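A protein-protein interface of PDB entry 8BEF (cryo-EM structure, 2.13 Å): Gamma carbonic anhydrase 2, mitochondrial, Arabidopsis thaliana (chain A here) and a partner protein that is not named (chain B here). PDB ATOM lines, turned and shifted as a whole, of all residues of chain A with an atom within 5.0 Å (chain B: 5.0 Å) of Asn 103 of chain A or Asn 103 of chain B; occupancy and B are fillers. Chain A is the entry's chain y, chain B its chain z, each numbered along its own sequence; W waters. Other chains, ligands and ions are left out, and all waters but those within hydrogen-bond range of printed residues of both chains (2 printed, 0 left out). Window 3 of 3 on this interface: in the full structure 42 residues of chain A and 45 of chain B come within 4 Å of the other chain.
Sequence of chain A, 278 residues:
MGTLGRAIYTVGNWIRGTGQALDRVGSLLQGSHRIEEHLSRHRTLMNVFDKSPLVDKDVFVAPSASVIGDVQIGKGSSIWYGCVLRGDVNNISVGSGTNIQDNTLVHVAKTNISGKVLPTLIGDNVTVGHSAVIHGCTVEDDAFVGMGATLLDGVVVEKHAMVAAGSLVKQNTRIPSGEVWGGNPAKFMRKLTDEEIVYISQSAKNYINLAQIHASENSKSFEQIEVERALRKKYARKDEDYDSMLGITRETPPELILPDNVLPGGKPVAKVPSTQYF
Asn 103 of chain A touches one residue of chain B. Of chain A, only Val 84, Asn 103, Thr 104 and Leu 105 come within 4 Å of Asn 103 of chain B. Printed residues of chain B within 4 Å of Val 84 of chain A: Asp 102 and Asn 103. Of the printed residues of chain B, Thr 104 of chain A touches Asn 103 (3.9 Å). Of the printed residues of chain A, Asp 102 of chain B touches Val 84 (3.2 Å) and Leu 105 (3.8 Å). Of the printed residues of chain B, Leu 105 of chain A touches Asp 102 and Asn 103. Cys 83 of chain A touches none of the printed residues of chain B. Cys 83 of chain B touches none of the printed residues of chain A. The nearest residue of chain A that does not touch Asn 103 of chain B is Gly 82 of chain A (4.1 Å). The nearest printed residue of chain B that does not touch Leu 105 of chain A is Ser 131 of chain B (4.2 Å).
O of Thr 104 of chain A lies within hydrogen-bond range of N of Val 84 of chain A, 2.9 Å away. The backbone NH of Ser 131 of chain A is in hydrogen-bond range of the side-chain hydroxyl of Thr 104 of chain A, at 3.4 Å. The side-chain hydroxyl of Thr 104 of chain A sits at hydrogen-bond distance from the backbone NH of Ala 132 of chain A, at 3.4 Å. The backbone NH (N) of Leu 105 of chain A is in hydrogen-bond range of the backbone carbonyl oxygen (O) of Ala 132 of chain A (3.0 Å). N of Tyr 81 of chain B lies within hydrogen-bond range of OD1 of Asp 102 of chain B, 2.6 Å away. The backbone carbonyl oxygen (O) of Tyr 81 of chain B is in hydrogen-bond range of the backbone NH (N) of Asn 103 of chain B (2.9 Å).
Among the printed residues, pairs that only touch across the chains: Val 84 of chain A with Asp 102 of chain B (3.2 Å), Val 84 of chain A with Asn 103 of chain B (3.7 Å), Asn 103 of chain A with Asn 103 of chain B (3.5 Å), Thr 104 of chain A with Asn 103 of chain B (3.9 Å), Leu 105 of chain A with Asp 102 of chain B (3.8 Å) and Leu 105 of chain A with Asn 103 of chain B (3.8 Å).
Water W1 lies within hydrogen-bond range of O of Asn 103 of chain A (2.8 Å), OG of Ser 131 of chain B (2.9 Å) and O of Ala 132 of chain A (3.2 Å). Water W2 bridges the backbone carbonyl oxygen of Gly 82 of chain A (2.9 Å) and the side-chain amide oxygen of Asn 103 of chain B (3.4 Å).
Printed residues of chain B that touch a printed residue of chain A: Asp 102 and Asn 103. Of the 11 printed residues of chain A, 4 touch a printed residue of chain B. Hydrophobic or aromatic side chains of chain A within 4 Å of the printed part of chain B: Val 84 and Leu 105. Among the printed residues, 6 pairs touch across the chains.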
ATOM      1  N   TYR A  81      -3.909  12.685 -20.139  1.00  0.00           N
ATOM      2  CA  TYR A  81      -4.682  12.909 -21.356  1.00  0.00           C
ATOM      3  C   TYR A  81      -4.311  14.232 -22.020  1.00  0.00           C
ATOM      4  O   TYR A  81      -4.255  15.275 -21.367  1.00  0.00           O
ATOM      5  CB  TYR A  81      -6.177  12.883 -21.028  1.00  0.00           C
ATOM      6  CG  TYR A  81      -6.612  11.605 -20.346  1.00  0.00           C
ATOM      7  CD1 TYR A  81      -6.785  10.432 -21.069  1.00  0.00           C
ATOM      8  CD2 TYR A  81      -6.810  11.565 -18.973  1.00  0.00           C
ATOM      9  CE1 TYR A  81      -7.168   9.262 -20.446  1.00  0.00           C
ATOM     10  CE2 TYR A  81      -7.190  10.404 -18.341  1.00  0.00           C
ATOM     11  CZ  TYR A  81      -7.368   9.253 -19.081  1.00  0.00           C
ATOM     12  OH  TYR A  81      -7.746   8.096 -18.454  1.00  0.00           O
ATOM     13  N   GLY A  82      -4.055  14.177 -23.325  1.00  0.00           N
ATOM     14  CA  GLY A  82      -3.782  15.366 -24.105  1.00  0.00           C
ATOM     15  C   GLY A  82      -2.380  15.921 -23.983  1.00  0.00           C
ATOM     16  O   GLY A  82      -2.089  16.952 -24.600  1.00  0.00           O
ATOM     17  N   CYS A  83      -1.508  15.288 -23.205  1.00  0.00           N
ATOM     18  CA  CYS A  83      -0.134  15.750 -23.087  1.00  0.00           C
ATOM     19  C   CYS A  83       0.616  15.578 -24.404  1.00  0.00           C
ATOM     20  O   CYS A  83       0.385  14.631 -25.157  1.00  0.00           O
ATOM     21  CB  CYS A  83       0.598  14.988 -21.983  1.00  0.00           C
ATOM     22  SG  CYS A  83      -0.115  15.156 -20.348  1.00  0.00           S
ATOM     23  N   VAL A  84       1.522  16.512 -24.676  1.00  0.00           N
ATOM     24  CA  VAL A  84       2.395  16.454 -25.842  1.00  0.00           C
ATOM     25  C   VAL A  84       3.834  16.548 -25.355  1.00  0.00           C
ATOM     26  O   VAL A  84       4.219  17.544 -24.731  1.00  0.00           O
ATOM     27  CB  VAL A  84       2.081  17.570 -26.852  1.00  0.00           C
ATOM     28  CG1 VAL A  84       3.025  17.494 -28.045  1.00  0.00           C
ATOM     29  CG2 VAL A  84       0.627  17.495 -27.304  1.00  0.00           C
ATOM     30  N   GLN A 101       0.725  16.228 -15.985  1.00  0.00           N
ATOM     31  CA  GLN A 101      -0.757  16.314 -15.992  1.00  0.00           C
ATOM     32  C   GLN A 101      -1.417  16.657 -17.348  1.00  0.00           C
ATOM     33  O   GLN A 101      -0.737  17.123 -18.211  1.00  0.00           O
ATOM     34  CB  GLN A 101      -1.273  17.178 -14.863  1.00  0.00           C
ATOM     35  CG  GLN A 101      -1.077  16.487 -13.511  1.00  0.00           C
ATOM     36  CD  GLN A 101      -1.335  17.356 -12.304  1.00  0.00           C
ATOM     37  OE1 GLN A 101      -2.122  18.288 -12.353  1.00  0.00           O
ATOM     38  NE2 GLN A 101      -0.675  17.047 -11.200  1.00  0.00           N
ATOM     39  N   ASP A 102      -2.728  16.636 -17.336  1.00  0.00           N
ATOM     40  CA  ASP A 102      -3.467  16.686 -18.593  1.00  0.00           C
ATOM     41  C   ASP A 102      -3.188  17.969 -19.369  1.00  0.00           C
ATOM     42  O   ASP A 102      -3.041  19.048 -18.789  1.00  0.00           O
ATOM     43  CB  ASP A 102      -4.965  16.575 -18.310  1.00  0.00           C
ATOM     44  CG  ASP A 102      -5.283  15.561 -17.224  1.00  0.00           C
ATOM     45  OD1 ASP A 102      -5.040  15.874 -16.041  1.00  0.00           O
ATOM     46  OD2 ASP A 102      -5.785  14.468 -17.544  1.00  0.00           O
ATOM     47  N   ASN A 103      -3.112  17.836 -20.693  1.00  0.00           N
ATOM     48  CA  ASN A 103      -3.015  18.954 -21.632  1.00  0.00           C
ATOM     49  C   ASN A 103      -1.723  19.754 -21.469  1.00  0.00           C
ATOM     50  O   ASN A 103      -1.665  20.923 -21.851  1.00  0.00           O
ATOM     51  CB  ASN A 103      -4.231  19.885 -21.514  1.00  0.00           C
ATOM     52  CG  ASN A 103      -5.453  19.357 -22.257  1.00  0.00           C
ATOM     53  OD1 ASN A 103      -5.431  18.265 -22.816  1.00  0.00           O
ATOM     54  ND2 ASN A 103      -6.527  20.138 -22.258  1.00  0.00           N
ATOM     55  N   THR A 104      -0.682  19.146 -20.907  1.00  0.00           N
ATOM     56  CA  THR A 104       0.611  19.803 -20.768  1.00  0.00           C
ATOM     57  C   THR A 104       1.424  19.668 -22.054  1.00  0.00           C
ATOM     58  O   THR A 104       1.350  18.658 -22.756  1.00  0.00           O
ATOM     59  CB  THR A 104       1.384  19.207 -19.582  1.00  0.00           C
ATOM     60  OG1 THR A 104       0.740  19.577 -18.355  1.00  0.00           O
ATOM     61  CG2 THR A 104       2.830  19.688 -19.546  1.00  0.00           C
ATOM     62  N   LEU A 105       2.191  20.708 -22.369  1.00  0.00           N
ATOM     63  CA  LEU A 105       3.121  20.691 -23.488  1.00  0.00           C
ATOM     64  C   LEU A 105       4.549  20.721 -22.960  1.00  0.00           C
ATOM     65  O   LEU A 105       4.906  21.599 -22.169  1.00  0.00           O
ATOM     66  CB  LEU A 105       2.877  21.876 -24.429  1.00  0.00           C
ATOM     67  CG  LEU A 105       3.743  22.042 -25.687  1.00  0.00           C
ATOM     68  CD1 LEU A 105       5.048  22.787 -25.398  1.00  0.00           C
ATOM     69  CD2 LEU A 105       4.018  20.703 -26.370  1.00  0.00           C
ATOM     70  N   SER A 131      -2.036  21.534 -17.928  1.00  0.00           N
ATOM     71  CA  SER A 131      -1.901  22.581 -18.945  1.00  0.00           C
ATOM     72  C   SER A 131      -0.678  23.463 -18.717  1.00  0.00           C
ATOM     73  O   SER A 131      -0.686  24.648 -19.052  1.00  0.00           O
ATOM     74  CB  SER A 131      -3.163  23.443 -19.028  1.00  0.00           C
ATOM     75  OG  SER A 131      -4.288  22.666 -19.387  1.00  0.00           O
ATOM     76  N   ALA A 132       0.379  22.903 -18.143  1.00  0.00           N
ATOM     77  CA  ALA A 132       1.626  23.639 -18.035  1.00  0.00           C
ATOM     78  C   ALA A 132       2.373  23.601 -19.365  1.00  0.00           C
ATOM     79  O   ALA A 132       2.080  22.793 -20.248  1.00  0.00           O
ATOM     80  CB  ALA A 132       2.501  23.066 -16.919  1.00  0.00           C
ATOM     81  N   TYR B  81       0.291  19.404 -32.865  1.00  0.00           N
ATOM     82  CA  TYR B  81      -0.477  18.440 -32.088  1.00  0.00           C
ATOM     83  C   TYR B  81      -1.346  19.129 -31.041  1.00  0.00           C
ATOM     84  O   TYR B  81      -0.878  19.990 -30.293  1.00  0.00           O
ATOM     85  CB  TYR B  81       0.479  17.445 -31.429  1.00  0.00           C
ATOM     86  CG  TYR B  81       1.331  16.694 -32.432  1.00  0.00           C
ATOM     87  CD1 TYR B  81       0.884  15.509 -33.003  1.00  0.00           C
ATOM     88  CD2 TYR B  81       2.574  17.182 -32.822  1.00  0.00           C
ATOM     89  CE1 TYR B  81       1.653  14.827 -33.924  1.00  0.00           C
ATOM     90  CE2 TYR B  81       3.347  16.509 -33.745  1.00  0.00           C
ATOM     91  CZ  TYR B  81       2.884  15.332 -34.295  1.00  0.00           C
ATOM     92  OH  TYR B  81       3.655  14.657 -35.210  1.00  0.00           O
ATOM     93  N   GLY B  82      -2.622  18.750 -31.002  1.00  0.00           N
ATOM     94  CA  GLY B  82      -3.558  19.260 -30.023  1.00  0.00           C
ATOM     95  C   GLY B  82      -4.178  20.604 -30.342  1.00  0.00           C
ATOM     96  O   GLY B  82      -4.980  21.100 -29.541  1.00  0.00           O
ATOM     97  N   CYS B  83      -3.836  21.213 -31.474  1.00  0.00           N
ATOM     98  CA  CYS B  83      -4.378  22.520 -31.816  1.00  0.00           C
ATOM     99  C   CYS B  83      -5.873  22.443 -32.102  1.00  0.00           C
ATOM    100  O   CYS B  83      -6.390  21.428 -32.573  1.00  0.00           O
ATOM    101  CB  CYS B  83      -3.657  23.098 -33.030  1.00  0.00           C
ATOM    102  SG  CYS B  83      -1.947  23.544 -32.735  1.00  0.00           S
ATOM    103  N   GLN B 101       1.549  26.387 -33.138  1.00  0.00           N
ATOM    104  CA  GLN B 101       2.199  25.396 -32.262  1.00  0.00           C
ATOM    105  C   GLN B 101       1.296  24.542 -31.373  1.00  0.00           C
ATOM    106  O   GLN B 101       0.194  24.913 -31.141  1.00  0.00           O
ATOM    107  CB  GLN B 101       3.389  26.049 -31.581  1.00  0.00           C
ATOM    108  CG  GLN B 101       4.513  26.349 -32.572  1.00  0.00           C
ATOM    109  CD  GLN B 101       5.638  27.070 -31.879  1.00  0.00           C
ATOM    110  OE1 GLN B 101       5.749  27.009 -30.667  1.00  0.00           O
ATOM    111  NE2 GLN B 101       6.474  27.759 -32.636  1.00  0.00           N
ATOM    112  N   ASP B 102       1.900  23.554 -30.765  1.00  0.00           N
ATOM    113  CA  ASP B 102       1.096  22.538 -30.094  1.00  0.00           C
ATOM    114  C   ASP B 102       0.169  23.133 -29.040  1.00  0.00           C
ATOM    115  O   ASP B 102       0.553  24.025 -28.280  1.00  0.00           O
ATOM    116  CB  ASP B 102       2.004  21.496 -29.441  1.00  0.00           C
ATOM    117  CG  ASP B 102       2.693  20.606 -30.453  1.00  0.00           C
ATOM    118  OD1 ASP B 102       2.268  20.596 -31.623  1.00  0.00           O
ATOM    119  OD2 ASP B 102       3.657  19.911 -30.077  1.00  0.00           O
ATOM    120  N   ASN B 103      -1.064  22.630 -29.048  1.00  0.00           N
ATOM    121  CA  ASN B 103      -2.070  23.002 -28.002  1.00  0.00           C
ATOM    122  C   ASN B 103      -2.540  24.461 -28.104  1.00  0.00           C
ATOM    123  O   ASN B 103      -3.156  24.910 -27.212  1.00  0.00           O
ATOM    124  CB  ASN B 103      -1.613  22.641 -26.570  1.00  0.00           C
ATOM    125  CG  ASN B 103      -1.356  21.157 -26.364  1.00  0.00           C
ATOM    126  OD1 ASN B 103      -1.733  20.321 -27.180  1.00  0.00           O
ATOM    127  ND2 ASN B 103      -0.715  20.807 -25.260  1.00  0.00           N
ATOM    128  N   SER B 104      -2.277  25.103 -29.215  1.00  0.00           N
ATOM    129  CA  SER B 104      -2.786  26.452 -29.403  1.00  0.00           C
ATOM    130  C   SER B 104      -4.265  26.419 -29.776  1.00  0.00           C
ATOM    131  O   SER B 104      -4.784  25.421 -30.280  1.00  0.00           O
ATOM    132  CB  SER B 104      -1.995  27.185 -30.484  1.00  0.00           C
ATOM    133  OG  SER B 104      -0.728  27.576 -29.996  1.00  0.00           O
ATOM    134  N   LEU B 105      -4.939  27.541 -29.493  1.00  0.00           N
ATOM    135  CA  LEU B 105      -6.370  27.691 -29.770  1.00  0.00           C
ATOM    136  C   LEU B 105      -6.625  28.965 -30.612  1.00  0.00           C
ATOM    137  O   LEU B 105      -6.335  30.047 -30.135  1.00  0.00           O
ATOM    138  CB  LEU B 105      -7.174  27.689 -28.476  1.00  0.00           C
ATOM    139  CG  LEU B 105      -8.658  28.045 -28.585  1.00  0.00           C
ATOM    140  CD1 LEU B 105      -9.436  26.978 -29.340  1.00  0.00           C
ATOM    141  CD2 LEU B 105      -9.261  28.261 -27.206  1.00  0.00           C
ATOM    142  N   SER B 131       0.362  26.720 -26.947  1.00  0.00           N
ATOM    143  CA  SER B 131      -0.712  27.010 -25.972  1.00  0.00           C
ATOM    144  C   SER B 131      -1.119  28.487 -25.956  1.00  0.00           C
ATOM    145  O   SER B 131      -1.561  28.927 -24.978  1.00  0.00           O
ATOM    146  CB  SER B 131      -0.340  26.459 -24.572  1.00  0.00           C
ATOM    147  OG  SER B 131       0.213  25.153 -24.645  1.00  0.00           O
ATOM    148  N   ALA B 132      -0.934  29.128 -27.068  1.00  0.00           N
ATOM    149  CA  ALA B 132      -1.434  30.483 -27.218  1.00  0.00           C
ATOM    150  C   ALA B 132      -2.927  30.459 -27.528  1.00  0.00           C
ATOM    151  O   ALA B 132      -3.464  29.483 -28.056  1.00  0.00           O
ATOM    152  CB  ALA B 132      -0.676  31.220 -28.322  1.00  0.00           C
HETATM  153  O   HOH W   1      -0.229  23.272 -22.451  1.00  0.00           O
HETATM  154  O   HOH W   2      -3.472  17.368 -27.159  1.00  0.00           O
